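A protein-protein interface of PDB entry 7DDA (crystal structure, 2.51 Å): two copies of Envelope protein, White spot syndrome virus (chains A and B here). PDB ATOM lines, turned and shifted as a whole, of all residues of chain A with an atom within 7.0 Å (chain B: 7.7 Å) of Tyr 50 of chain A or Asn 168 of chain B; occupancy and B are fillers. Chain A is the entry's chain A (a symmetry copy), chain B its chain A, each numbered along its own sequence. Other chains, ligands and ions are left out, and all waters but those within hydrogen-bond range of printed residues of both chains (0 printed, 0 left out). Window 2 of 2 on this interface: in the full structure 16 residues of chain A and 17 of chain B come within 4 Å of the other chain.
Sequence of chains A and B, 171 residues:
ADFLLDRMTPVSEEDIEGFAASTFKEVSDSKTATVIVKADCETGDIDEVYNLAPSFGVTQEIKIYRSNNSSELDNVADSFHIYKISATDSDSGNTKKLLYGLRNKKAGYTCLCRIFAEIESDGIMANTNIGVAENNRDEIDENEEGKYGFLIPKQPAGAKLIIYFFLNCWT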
ATOM      1  N   THR A  34      23.435 -11.650  -1.573  1.00  0.00           N
ATOM      2  CA  THR A  34      22.043 -11.617  -1.151  1.00  0.00           C
ATOM      3  C   THR A  34      21.181 -11.625  -2.401  1.00  0.00           C
ATOM      4  O   THR A  34      21.374 -10.789  -3.291  1.00  0.00           O
ATOM      5  CB  THR A  34      21.741 -10.364  -0.315  1.00  0.00           C
ATOM      6  OG1 THR A  34      22.571 -10.359   0.853  1.00  0.00           O
ATOM      7  CG2 THR A  34      20.267 -10.312   0.084  1.00  0.00           C
ATOM      8  N   VAL A  35      20.244 -12.563  -2.477  1.00  0.00           N
ATOM      9  CA  VAL A  35      19.352 -12.681  -3.623  1.00  0.00           C
ATOM     10  C   VAL A  35      17.916 -12.597  -3.113  1.00  0.00           C
ATOM     11  O   VAL A  35      17.509 -13.380  -2.242  1.00  0.00           O
ATOM     12  CB  VAL A  35      19.614 -13.981  -4.409  1.00  0.00           C
ATOM     13  CG1 VAL A  35      18.798 -14.025  -5.692  1.00  0.00           C
ATOM     14  CG2 VAL A  35      21.096 -14.108  -4.726  1.00  0.00           C
ATOM     15  N   ILE A  36      17.156 -11.641  -3.647  1.00  0.00           N
ATOM     16  CA  ILE A  36      15.780 -11.376  -3.232  1.00  0.00           C
ATOM     17  C   ILE A  36      14.856 -11.905  -4.318  1.00  0.00           C
ATOM     18  O   ILE A  36      14.902 -11.446  -5.466  1.00  0.00           O
ATOM     19  CB  ILE A  36      15.546  -9.877  -2.982  1.00  0.00           C
ATOM     20  CG1 ILE A  36      16.583  -9.320  -2.005  1.00  0.00           C
ATOM     21  CG2 ILE A  36      14.146  -9.620  -2.433  1.00  0.00           C
ATOM     22  CD1 ILE A  36      16.426  -7.813  -1.742  1.00  0.00           C
ATOM     23  N   VAL A  37      14.037 -12.888  -3.969  1.00  0.00           N
ATOM     24  CA  VAL A  37      13.166 -13.564  -4.922  1.00  0.00           C
ATOM     25  C   VAL A  37      11.731 -13.184  -4.597  1.00  0.00           C
ATOM     26  O   VAL A  37      11.296 -13.316  -3.443  1.00  0.00           O
ATOM     27  CB  VAL A  37      13.341 -15.092  -4.873  1.00  0.00           C
ATOM     28  CG1 VAL A  37      12.275 -15.786  -5.736  1.00  0.00           C
ATOM     29  CG2 VAL A  37      14.751 -15.491  -5.287  1.00  0.00           C
ATOM     30  N   LYS A  38      11.006 -12.711  -5.617  1.00  0.00           N
ATOM     31  CA  LYS A  38       9.576 -12.455  -5.537  1.00  0.00           C
ATOM     32  C   LYS A  38       8.816 -13.592  -6.221  1.00  0.00           C
ATOM     33  O   LYS A  38       9.026 -13.857  -7.413  1.00  0.00           O
ATOM     34  CB  LYS A  38       9.228 -11.112  -6.178  1.00  0.00           C
ATOM     35  CG  LYS A  38       7.728 -10.874  -6.258  1.00  0.00           C
ATOM     36  CD  LYS A  38       7.379  -9.396  -6.304  1.00  0.00           C
ATOM     37  CE  LYS A  38       7.331  -8.866  -7.711  1.00  0.00           C
ATOM     38  NZ  LYS A  38       6.035  -9.205  -8.339  1.00  0.00           N
ATOM     39  N   GLU A  48      10.555 -12.707 -10.109  1.00  0.00           N
ATOM     40  CA  GLU A  48      11.768 -11.916 -10.230  1.00  0.00           C
ATOM     41  C   GLU A  48      12.851 -12.500  -9.330  1.00  0.00           C
ATOM     42  O   GLU A  48      12.567 -12.938  -8.211  1.00  0.00           O
ATOM     43  CB  GLU A  48      11.514 -10.442  -9.859  1.00  0.00           C
ATOM     44  CG  GLU A  48      12.773  -9.603  -9.877  1.00  0.00           C
ATOM     45  CD  GLU A  48      12.544  -8.166  -9.488  1.00  0.00           C
ATOM     46  OE1 GLU A  48      12.379  -7.873  -8.294  1.00  0.00           O
ATOM     47  OE2 GLU A  48      12.554  -7.312 -10.383  1.00  0.00           O
ATOM     48  N   VAL A  49      14.085 -12.496  -9.836  1.00  0.00           N
ATOM     49  CA  VAL A  49      15.283 -12.880  -9.099  1.00  0.00           C
ATOM     50  C   VAL A  49      16.207 -11.670  -9.093  1.00  0.00           C
ATOM     51  O   VAL A  49      16.801 -11.330 -10.119  1.00  0.00           O
ATOM     52  CB  VAL A  49      15.968 -14.106  -9.719  1.00  0.00           C
ATOM     53  CG1 VAL A  49      17.209 -14.494  -8.919  1.00  0.00           C
ATOM     54  CG2 VAL A  49      14.990 -15.262  -9.780  1.00  0.00           C
ATOM     55  N   TYR A  50      16.336 -11.022  -7.941  1.00  0.00           N
ATOM     56  CA  TYR A  50      17.001  -9.729  -7.812  1.00  0.00           C
ATOM     57  C   TYR A  50      18.300  -9.931  -7.044  1.00  0.00           C
ATOM     58  O   TYR A  50      18.276 -10.287  -5.863  1.00  0.00           O
ATOM     59  CB  TYR A  50      16.057  -8.759  -7.108  1.00  0.00           C
ATOM     60  CG  TYR A  50      16.518  -7.333  -6.935  1.00  0.00           C
ATOM     61  CD1 TYR A  50      16.352  -6.403  -7.948  1.00  0.00           C
ATOM     62  CD2 TYR A  50      17.062  -6.899  -5.727  1.00  0.00           C
ATOM     63  CE1 TYR A  50      16.733  -5.090  -7.773  1.00  0.00           C
ATOM     64  CE2 TYR A  50      17.451  -5.596  -5.551  1.00  0.00           C
ATOM     65  CZ  TYR A  50      17.286  -4.692  -6.579  1.00  0.00           C
ATOM     66  OH  TYR A  50      17.669  -3.382  -6.401  1.00  0.00           O
ATOM     67  N   ASN A  51      19.431  -9.720  -7.708  1.00  0.00           N
ATOM     68  CA  ASN A  51      20.741 -10.021  -7.133  1.00  0.00           C
ATOM     69  C   ASN A  51      21.380  -8.766  -6.556  1.00  0.00           C
ATOM     70  O   ASN A  51      21.412  -7.722  -7.212  1.00  0.00           O
ATOM     71  CB  ASN A  51      21.661 -10.650  -8.184  1.00  0.00           C
ATOM     72  CG  ASN A  51      21.009 -11.837  -8.899  1.00  0.00           C
ATOM     73  OD1 ASN A  51      20.720 -12.858  -8.277  1.00  0.00           O
ATOM     74  ND2 ASN A  51      20.764 -11.700 -10.201  1.00  0.00           N
ATOM     75  N   LEU A  52      21.884  -8.872  -5.325  1.00  0.00           N
ATOM     76  CA  LEU A  52      22.639  -7.800  -4.676  1.00  0.00           C
ATOM     77  C   LEU A  52      24.131  -8.088  -4.841  1.00  0.00           C
ATOM     78  O   LEU A  52      24.663  -9.024  -4.232  1.00  0.00           O
ATOM     79  CB  LEU A  52      22.264  -7.676  -3.203  1.00  0.00           C
ATOM     80  CG  LEU A  52      21.153  -6.681  -2.862  1.00  0.00           C
ATOM     81  CD1 LEU A  52      20.016  -6.822  -3.835  1.00  0.00           C
ATOM     82  CD2 LEU A  52      20.656  -6.849  -1.428  1.00  0.00           C
ATOM     83  N   ALA A  53      24.796  -7.279  -5.663  1.00  0.00           N
ATOM     84  CA  ALA A  53      26.188  -7.493  -6.065  1.00  0.00           C
ATOM     85  C   ALA A  53      26.317  -8.784  -6.873  1.00  0.00           C
ATOM     86  O   ALA A  53      26.323  -8.752  -8.110  1.00  0.00           O
ATOM     87  CB  ALA A  53      27.126  -7.509  -4.844  1.00  0.00           C
ATOM     88  N   VAL A  76      26.679 -13.752 -10.077  1.00  0.00           N
ATOM     89  CA  VAL A  76      25.645 -13.809  -9.050  1.00  0.00           C
ATOM     90  C   VAL A  76      24.316 -14.232  -9.677  1.00  0.00           C
ATOM     91  O   VAL A  76      23.506 -14.917  -9.041  1.00  0.00           O
ATOM     92  CB  VAL A  76      25.516 -12.458  -8.305  1.00  0.00           C
ATOM     93  CG1 VAL A  76      24.468 -12.541  -7.207  1.00  0.00           C
ATOM     94  CG2 VAL A  76      26.853 -12.056  -7.712  1.00  0.00           C
ATOM     95  N   ILE A  82      17.534 -20.505  -9.006  1.00  0.00           N
ATOM     96  CA  ILE A  82      16.448 -20.592  -8.033  1.00  0.00           C
ATOM     97  C   ILE A  82      15.162 -20.907  -8.783  1.00  0.00           C
ATOM     98  O   ILE A  82      14.859 -20.277  -9.805  1.00  0.00           O
ATOM     99  CB  ILE A  82      16.309 -19.291  -7.220  1.00  0.00           C
ATOM    100  CG1 ILE A  82      17.651 -18.932  -6.574  1.00  0.00           C
ATOM    101  CG2 ILE A  82      15.207 -19.430  -6.166  1.00  0.00           C
ATOM    102  CD1 ILE A  82      17.793 -17.456  -6.233  1.00  0.00           C
ATOM    103  N   SER B  30      29.336  -1.061 -11.474  1.00  0.00           N
ATOM    104  CA  SER B  30      28.097  -1.507 -10.844  1.00  0.00           C
ATOM    105  C   SER B  30      28.237  -1.445  -9.325  1.00  0.00           C
ATOM    106  O   SER B  30      29.298  -1.761  -8.782  1.00  0.00           O
ATOM    107  CB  SER B  30      27.735  -2.931 -11.286  1.00  0.00           C
ATOM    108  OG  SER B  30      26.584  -3.393 -10.601  1.00  0.00           O
ATOM    109  N   LYS B  31      27.169  -1.036  -8.640  1.00  0.00           N
ATOM    110  CA  LYS B  31      27.221  -0.795  -7.201  1.00  0.00           C
ATOM    111  C   LYS B  31      25.895  -1.179  -6.550  1.00  0.00           C
ATOM    112  O   LYS B  31      24.828  -1.106  -7.172  1.00  0.00           O
ATOM    113  CB  LYS B  31      27.531   0.680  -6.884  1.00  0.00           C
ATOM    114  CG  LYS B  31      28.839   1.197  -7.444  1.00  0.00           C
ATOM    115  CD  LYS B  31      29.887   1.372  -6.362  1.00  0.00           C
ATOM    116  CE  LYS B  31      30.933   2.387  -6.791  1.00  0.00           C
ATOM    117  NZ  LYS B  31      32.208   2.207  -6.056  1.00  0.00           N
ATOM    118  N   THR B  32      25.976  -1.596  -5.286  1.00  0.00           N
ATOM    119  CA  THR B  32      24.798  -1.853  -4.472  1.00  0.00           C
ATOM    120  C   THR B  32      24.965  -1.222  -3.093  1.00  0.00           C
ATOM    121  O   THR B  32      26.081  -1.085  -2.579  1.00  0.00           O
ATOM    122  CB  THR B  32      24.483  -3.354  -4.309  1.00  0.00           C
ATOM    123  OG1 THR B  32      25.612  -4.032  -3.745  1.00  0.00           O
ATOM    124  CG2 THR B  32      24.101  -4.014  -5.619  1.00  0.00           C
ATOM    125  N   ALA B  33      23.838  -0.816  -2.510  1.00  0.00           N
ATOM    126  CA  ALA B  33      23.816  -0.253  -1.168  1.00  0.00           C
ATOM    127  C   ALA B  33      22.510  -0.635  -0.486  1.00  0.00           C
ATOM    128  O   ALA B  33      21.479  -0.848  -1.139  1.00  0.00           O
ATOM    129  CB  ALA B  33      23.981   1.269  -1.179  1.00  0.00           C
ATOM    130  N   THR B  34      22.573  -0.728   0.836  1.00  0.00           N
ATOM    131  CA  THR B  34      21.417  -0.932   1.696  1.00  0.00           C
ATOM    132  C   THR B  34      21.295   0.281   2.601  1.00  0.00           C
ATOM    133  O   THR B  34      22.262   0.650   3.274  1.00  0.00           O
ATOM    134  CB  THR B  34      21.566  -2.205   2.542  1.00  0.00           C
ATOM    135  OG1 THR B  34      21.697  -3.339   1.679  1.00  0.00           O
ATOM    136  CG2 THR B  34      20.369  -2.387   3.475  1.00  0.00           C
ATOM    137  N   PHE B  80      22.009   9.344  -2.452  1.00  0.00           N
ATOM    138  CA  PHE B  80      20.566   9.198  -2.428  1.00  0.00           C
ATOM    139  C   PHE B  80      19.992  10.234  -1.487  1.00  0.00           C
ATOM    140  O   PHE B  80      20.668  10.696  -0.566  1.00  0.00           O
ATOM    141  CB  PHE B  80      20.160   7.793  -1.989  1.00  0.00           C
ATOM    142  CG  PHE B  80      20.795   6.726  -2.803  1.00  0.00           C
ATOM    143  CD1 PHE B  80      20.418   6.535  -4.131  1.00  0.00           C
ATOM    144  CD2 PHE B  80      21.819   5.946  -2.274  1.00  0.00           C
ATOM    145  CE1 PHE B  80      21.026   5.550  -4.914  1.00  0.00           C
ATOM    146  CE2 PHE B  80      22.434   4.966  -3.042  1.00  0.00           C
ATOM    147  CZ  PHE B  80      22.038   4.767  -4.366  1.00  0.00           C
ATOM    148  N   ASN B 104      17.475   9.197  -6.807  1.00  0.00           N
ATOM    149  CA  ASN B 104      18.815   8.866  -7.268  1.00  0.00           C
ATOM    150  C   ASN B 104      19.601  10.159  -7.480  1.00  0.00           C
ATOM    151  O   ASN B 104      19.215  11.007  -8.290  1.00  0.00           O
ATOM    152  CB  ASN B 104      18.721   8.037  -8.551  1.00  0.00           C
ATOM    153  CG  ASN B 104      20.092   7.688  -9.155  1.00  0.00           C
ATOM    154  OD1 ASN B 104      21.156   7.997  -8.599  1.00  0.00           O
ATOM    155  ND2 ASN B 104      20.058   7.024 -10.305  1.00  0.00           N
ATOM    156  N   TYR B 109      24.482   7.253 -12.983  1.00  0.00           N
ATOM    157  CA  TYR B 109      23.933   5.953 -12.613  1.00  0.00           C
ATOM    158  C   TYR B 109      22.427   5.854 -12.825  1.00  0.00           C
ATOM    159  O   TYR B 109      21.683   6.820 -12.633  1.00  0.00           O
ATOM    160  CB  TYR B 109      24.256   5.626 -11.160  1.00  0.00           C
ATOM    161  CG  TYR B 109      25.691   5.210 -10.934  1.00  0.00           C
ATOM    162  CD1 TYR B 109      26.706   6.156 -10.823  1.00  0.00           C
ATOM    163  CD2 TYR B 109      26.033   3.863 -10.832  1.00  0.00           C
ATOM    164  CE1 TYR B 109      28.022   5.766 -10.611  1.00  0.00           C
ATOM    165  CE2 TYR B 109      27.341   3.466 -10.616  1.00  0.00           C
ATOM    166  CZ  TYR B 109      28.330   4.418 -10.507  1.00  0.00           C
ATOM    167  OH  TYR B 109      29.623   4.010 -10.294  1.00  0.00           O
ATOM    168  N   THR B 110      21.999   4.669 -13.239  1.00  0.00           N
ATOM    169  CA  THR B 110      20.613   4.236 -13.214  1.00  0.00           C
ATOM    170  C   THR B 110      20.472   3.240 -12.072  1.00  0.00           C
ATOM    171  O   THR B 110      21.414   2.494 -11.783  1.00  0.00           O
ATOM    172  CB  THR B 110      20.226   3.592 -14.549  1.00  0.00           C
ATOM    173  OG1 THR B 110      20.497   4.520 -15.607  1.00  0.00           O
ATOM    174  CG2 THR B 110      18.742   3.203 -14.582  1.00  0.00           C
ATOM    175  N   CYS B 111      19.315   3.235 -11.397  1.00  0.00           N
ATOM    176  CA  CYS B 111      19.163   2.413 -10.206  1.00  0.00           C
ATOM    177  C   CYS B 111      17.864   1.624 -10.217  1.00  0.00           C
ATOM    178  O   CYS B 111      16.850   2.047 -10.783  1.00  0.00           O
ATOM    179  CB  CYS B 111      19.219   3.240  -8.923  1.00  0.00           C
ATOM    180  SG  CYS B 111      20.798   4.050  -8.603  1.00  0.00           S
ATOM    181  N   LEU B 112      17.925   0.461  -9.578  1.00  0.00           N
ATOM    182  CA  LEU B 112      16.755  -0.267  -9.124  1.00  0.00           C
ATOM    183  C   LEU B 112      16.675  -0.192  -7.599  1.00  0.00           C
ATOM    184  O   LEU B 112      17.695  -0.051  -6.908  1.00  0.00           O
ATOM    185  CB  LEU B 112      16.806  -1.718  -9.594  1.00  0.00           C
ATOM    186  CG  LEU B 112      16.560  -1.976 -11.081  1.00  0.00           C
ATOM    187  CD1 LEU B 112      16.786  -3.442 -11.365  1.00  0.00           C
ATOM    188  CD2 LEU B 112      15.147  -1.567 -11.522  1.00  0.00           C
ATOM    189  N   CYS B 113      15.450  -0.274  -7.079  1.00  0.00           N
ATOM    190  CA  CYS B 113      15.207  -0.211  -5.644  1.00  0.00           C
ATOM    191  C   CYS B 113      14.184  -1.268  -5.260  1.00  0.00           C
ATOM    192  O   CYS B 113      13.083  -1.299  -5.821  1.00  0.00           O
ATOM    193  CB  CYS B 113      14.705   1.174  -5.232  1.00  0.00           C
ATOM    194  SG  CYS B 113      14.715   1.466  -3.457  1.00  0.00           S
ATOM    195  N   ARG B 114      14.532  -2.122  -4.298  1.00  0.00           N
ATOM    196  CA  ARG B 114      13.573  -3.021  -3.668  1.00  0.00           C
ATOM    197  C   ARG B 114      13.528  -2.717  -2.174  1.00  0.00           C
ATOM    198  O   ARG B 114      14.521  -2.259  -1.596  1.00  0.00           O
ATOM    199  CB  ARG B 114      13.933  -4.491  -3.905  1.00  0.00           C
ATOM    200  CG  ARG B 114      13.976  -4.897  -5.366  1.00  0.00           C
ATOM    201  CD  ARG B 114      12.594  -4.886  -5.954  1.00  0.00           C
ATOM    202  NE  ARG B 114      12.596  -5.122  -7.398  1.00  0.00           N
ATOM    203  CZ  ARG B 114      12.825  -4.178  -8.315  1.00  0.00           C
ATOM    204  NH1 ARG B 114      13.104  -2.929  -7.941  1.00  0.00           N
ATOM    205  NH2 ARG B 114      12.785  -4.485  -9.609  1.00  0.00           N
ATOM    206  N   ILE B 115      12.370  -2.973  -1.544  1.00  0.00           N
ATOM    207  CA  ILE B 115      12.134  -2.521  -0.180  1.00  0.00           C
ATOM    208  C   ILE B 115      11.628  -3.639   0.722  1.00  0.00           C
ATOM    209  O   ILE B 115      11.010  -4.619   0.291  1.00  0.00           O
ATOM    210  CB  ILE B 115      11.131  -1.356  -0.102  1.00  0.00           C
ATOM    211  CG1 ILE B 115       9.754  -1.876  -0.477  1.00  0.00           C
ATOM    212  CG2 ILE B 115      11.588  -0.147  -0.937  1.00  0.00           C
ATOM    213  CD1 ILE B 115       8.670  -0.916  -0.249  1.00  0.00           C
ATOM    214  N   ARG B 137       9.164  -0.258  -9.106  1.00  0.00           N
ATOM    215  CA  ARG B 137      10.007  -1.400  -9.433  1.00  0.00           C
ATOM    216  C   ARG B 137      10.882  -1.159 -10.652  1.00  0.00           C
ATOM    217  O   ARG B 137      11.668  -2.038 -11.017  1.00  0.00           O
ATOM    218  CB  ARG B 137       9.134  -2.639  -9.672  1.00  0.00           C
ATOM    219  CG  ARG B 137       8.437  -3.070  -8.425  1.00  0.00           C
ATOM    220  CD  ARG B 137       7.174  -3.829  -8.684  1.00  0.00           C
ATOM    221  NE  ARG B 137       6.602  -4.294  -7.418  1.00  0.00           N
ATOM    222  CZ  ARG B 137       7.185  -5.149  -6.575  1.00  0.00           C
ATOM    223  NH1 ARG B 137       8.359  -5.714  -6.861  1.00  0.00           N
ATOM    224  NH2 ARG B 137       6.566  -5.462  -5.447  1.00  0.00           N
ATOM    225  N   GLU B 139      13.438   1.161 -13.468  1.00  0.00           N
ATOM    226  CA  GLU B 139      14.682   1.901 -13.415  1.00  0.00           C
ATOM    227  C   GLU B 139      14.422   3.319 -12.917  1.00  0.00           C
ATOM    228  O   GLU B 139      13.340   3.878 -13.106  1.00  0.00           O
ATOM    229  CB  GLU B 139      15.328   1.911 -14.793  1.00  0.00           C
ATOM    230  CG  GLU B 139      15.718   0.526 -15.247  1.00  0.00           C
ATOM    231  CD  GLU B 139      16.572   0.544 -16.491  1.00  0.00           C
ATOM    232  OE1 GLU B 139      16.867  -0.550 -17.030  1.00  0.00           O
ATOM    233  OE2 GLU B 139      16.946   1.656 -16.919  1.00  0.00           O
ATOM    234  N   ILE B 140      15.412   3.884 -12.238  1.00  0.00           N
ATOM    235  CA  ILE B 140      15.308   5.213 -11.656  1.00  0.00           C
ATOM    236  C   ILE B 140      16.540   5.968 -12.114  1.00  0.00           C
ATOM    237  O   ILE B 140      17.651   5.696 -11.642  1.00  0.00           O
ATOM    238  CB  ILE B 140      15.218   5.193 -10.121  1.00  0.00           C
ATOM    239  CG1 ILE B 140      13.962   4.450  -9.645  1.00  0.00           C
ATOM    240  CG2 ILE B 140      15.185   6.604  -9.567  1.00  0.00           C
ATOM    241  CD1 ILE B 140      13.971   4.153  -8.144  1.00  0.00           C
ATOM    242  N   PHE B 165      15.947  -0.083   2.077  1.00  0.00           N
ATOM    243  CA  PHE B 165      16.063   0.149   0.643  1.00  0.00           C
ATOM    244  C   PHE B 165      17.244  -0.652   0.127  1.00  0.00           C
ATOM    245  O   PHE B 165      18.382  -0.435   0.568  1.00  0.00           O
ATOM    246  CB  PHE B 165      16.258   1.634   0.335  1.00  0.00           C
ATOM    247  CG  PHE B 165      15.125   2.502   0.791  1.00  0.00           C
ATOM    248  CD1 PHE B 165      15.053   2.937   2.108  1.00  0.00           C
ATOM    249  CD2 PHE B 165      14.148   2.897  -0.089  1.00  0.00           C
ATOM    250  CE1 PHE B 165      14.009   3.740   2.527  1.00  0.00           C
ATOM    251  CE2 PHE B 165      13.116   3.699   0.326  1.00  0.00           C
ATOM    252  CZ  PHE B 165      13.043   4.121   1.629  1.00  0.00           C
ATOM    253  N   PHE B 166      16.973  -1.564  -0.809  1.00  0.00           N
ATOM    254  CA  PHE B 166      18.006  -2.403  -1.422  1.00  0.00           C
ATOM    255  C   PHE B 166      18.287  -1.860  -2.816  1.00  0.00           C
ATOM    256  O   PHE B 166      17.521  -2.100  -3.755  1.00  0.00           O
ATOM    257  CB  PHE B 166      17.578  -3.862  -1.446  1.00  0.00           C
ATOM    258  CG  PHE B 166      17.163  -4.383  -0.091  1.00  0.00           C
ATOM    259  CD1 PHE B 166      18.105  -4.562   0.910  1.00  0.00           C
ATOM    260  CD2 PHE B 166      15.834  -4.650   0.194  1.00  0.00           C
ATOM    261  CE1 PHE B 166      17.738  -5.035   2.155  1.00  0.00           C
ATOM    262  CE2 PHE B 166      15.465  -5.117   1.432  1.00  0.00           C
ATOM    263  CZ  PHE B 166      16.417  -5.317   2.417  1.00  0.00           C
ATOM    264  N   LEU B 167      19.406  -1.145  -2.942  1.00  0.00           N
ATOM    265  CA  LEU B 167      19.716  -0.347  -4.121  1.00  0.00           C
ATOM    266  C   LEU B 167      20.737  -1.050  -5.011  1.00  0.00           C
ATOM    267  O   LEU B 167      21.773  -1.524  -4.534  1.00  0.00           O
ATOM    268  CB  LEU B 167      20.219   1.025  -3.679  1.00  0.00           C
ATOM    269  CG  LEU B 167      19.069   1.873  -3.137  1.00  0.00           C
ATOM    270  CD1 LEU B 167      19.591   2.938  -2.210  1.00  0.00           C
ATOM    271  CD2 LEU B 167      18.317   2.533  -4.288  1.00  0.00           C
ATOM    272  N   ASN B 168      20.430  -1.120  -6.303  1.00  0.00           N
ATOM    273  CA  ASN B 168      21.316  -1.725  -7.291  1.00  0.00           C
ATOM    274  C   ASN B 168      21.480  -0.750  -8.447  1.00  0.00           C
ATOM    275  O   ASN B 168      20.550  -0.557  -9.234  1.00  0.00           O
ATOM    276  CB  ASN B 168      20.774  -3.070  -7.773  1.00  0.00           C
ATOM    277  CG  ASN B 168      21.738  -3.781  -8.700  1.00  0.00           C
ATOM    278  OD1 ASN B 168      21.342  -4.645  -9.482  1.00  0.00           O
ATOM    279  ND2 ASN B 168      23.010  -3.386  -8.649  1.00  0.00           N
ATOM    280  N   CYS B 169      22.661  -0.149  -8.553  1.00  0.00           N
ATOM    281  CA  CYS B 169      22.920   0.926  -9.496  1.00  0.00           C
ATOM    282  C   CYS B 169      24.076   0.579 -10.433  1.00  0.00           C
ATOM    283  O   CYS B 169      25.004  -0.150 -10.065  1.00  0.00           O
ATOM    284  CB  CYS B 169      23.232   2.223  -8.752  1.00  0.00           C
ATOM    285  SG  CYS B 169      21.939   2.684  -7.611  1.00  0.00           S
ATOM    286  N   TRP B 170      24.022   1.132 -11.646  1.00  0.00           N
ATOM    287  CA  TRP B 170      25.025   0.859 -12.663  1.00  0.00           C
ATOM    288  C   TRP B 170      25.126   2.047 -13.614  1.00  0.00           C
ATOM    289  O   TRP B 170      24.263   2.923 -13.633  1.00  0.00           O
ATOM    290  CB  TRP B 170      24.684  -0.418 -13.426  1.00  0.00           C
ATOM    291  CG  TRP B 170      23.429  -0.301 -14.199  1.00  0.00           C
ATOM    292  CD1 TRP B 170      23.302   0.143 -15.475  1.00  0.00           C
ATOM    293  CD2 TRP B 170      22.104  -0.628 -13.752  1.00  0.00           C
ATOM    294  NE1 TRP B 170      21.978   0.119 -15.857  1.00  0.00           N
ATOM    295  CE2 TRP B 170      21.223  -0.351 -14.815  1.00  0.00           C
ATOM    296  CE3 TRP B 170      21.579  -1.122 -12.556  1.00  0.00           C
ATOM    297  CZ2 TRP B 170      19.848  -0.561 -14.722  1.00  0.00           C
ATOM    298  CZ3 TRP B 170      20.212  -1.326 -12.468  1.00  0.00           C
ATOM    299  CH2 TRP B 170      19.365  -1.047 -13.545  1.00  0.00           C
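1 position is printed for both chains.
Among the printed residues, pairs that only touch across the chains: Ala 53 of chain A with Thr 32 of chain B, Tyr 50 of chain A with Asn 168 of chain B, Lys 38 of chain A with Arg 137 of chain B, Tyr 50 of chain A with Arg 114 of chain B, Ile 36 of chain A with Phe 166 of chain B, Asn 51 of chain A with Asn 168 of chain B and Tyr 50 of chain A with Cys 113 of chain B.
Val 37 of chain A touches none of the printed residues of chain B.
Tyr 50 of chain A touches five residues of chain B.
Printed residues of chain A within 4 Å of Thr 32 of chain B: Ala 53.
Of the printed residues of chain A, Cys 113 of chain B touches Tyr 50.
Of the printed residues of chain A, Phe 166 of chain B touches Ile 36 and Tyr 50.
Of chain A, only Tyr 50 and Asn 51 come within 4 Å of Asn 168 of chain B.
The nearest residue of chain B that does not touch Tyr 50 of chain A is Leu 167 of chain B (4.1 Å).
The nearest printed residue of chain B that does not touch Asn 51 of chain A is Thr 32 of chain B (4.8 Å).
The side-chain hydroxyl of Tyr 50 of chain A lies within hydrogen-bond range of the backbone carbonyl oxygen of Leu 112 of chain B (3.4 Å).
The guanidinium group (NE) of Arg 114 of chain B lies within salt-bridge range of the side-chain carboxylate (OE1) of Glu 48 of chain A (2.9 Å).
The backbone carbonyl oxygen (O) of Phe 166 of chain B lies within hydrogen-bond range of the side-chain hydroxyl (OH) of Tyr 50 of chain A, at 2.9 Å.
Of the 13 printed residues of chain A, 6 touch a printed residue of chain B.
Hydrophobic or aromatic side chains of chain A within 4 Å of the printed part of chain B: Ile 36, Tyr 50 and Ala 53.
Of the 23 printed residues of chain B, 7 touch a printed residue of chain A.
Printed residues of chain B that touch a printed residue of chain A: Thr 32, Leu 112, Cys 113, Arg 114, Arg 137, Phe 166 and Asn 168.
Hydrophobic or aromatic side chains of chain B that line the printed part of chain A: Leu 112 and Phe 166.
Among the printed residues, 10 pairs touch across the chains.
Among the printed residues, Asp or Glu carboxylates within 4 Å of a Lys or Arg side-chain nitrogen of the other chain: Glu 48 of chain A with Arg 114 of chain B (2.9 Å).
The backbone NH of Leu 112 of chain B is in hydrogen-bond range of the backbone carbonyl oxygen of Asn 168 of chain B.
NH2 of Arg 114 of chain B lies within hydrogen-bond range of O of Arg 137 of chain B (3.0 Å).
The backbone NH of Phe 166 of chain B is in hydrogen-bond range of the backbone carbonyl oxygen of Arg 114 of chain B.
The backbone NH of Ile 36 of chain A sits at hydrogen-bond distance from the backbone carbonyl oxygen of Tyr 50 of chain A (2.8 Å).
The backbone carbonyl oxygen of Glu 48 of chain A is in hydrogen-bond range of the backbone NH of Lys 38 of chain A.
The side-chain sulfur (SG) of Cys 111 of chain B is disulfide-bonded to the side-chain sulfur (SG) of Cys 169 of chain B (2.0 Å).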
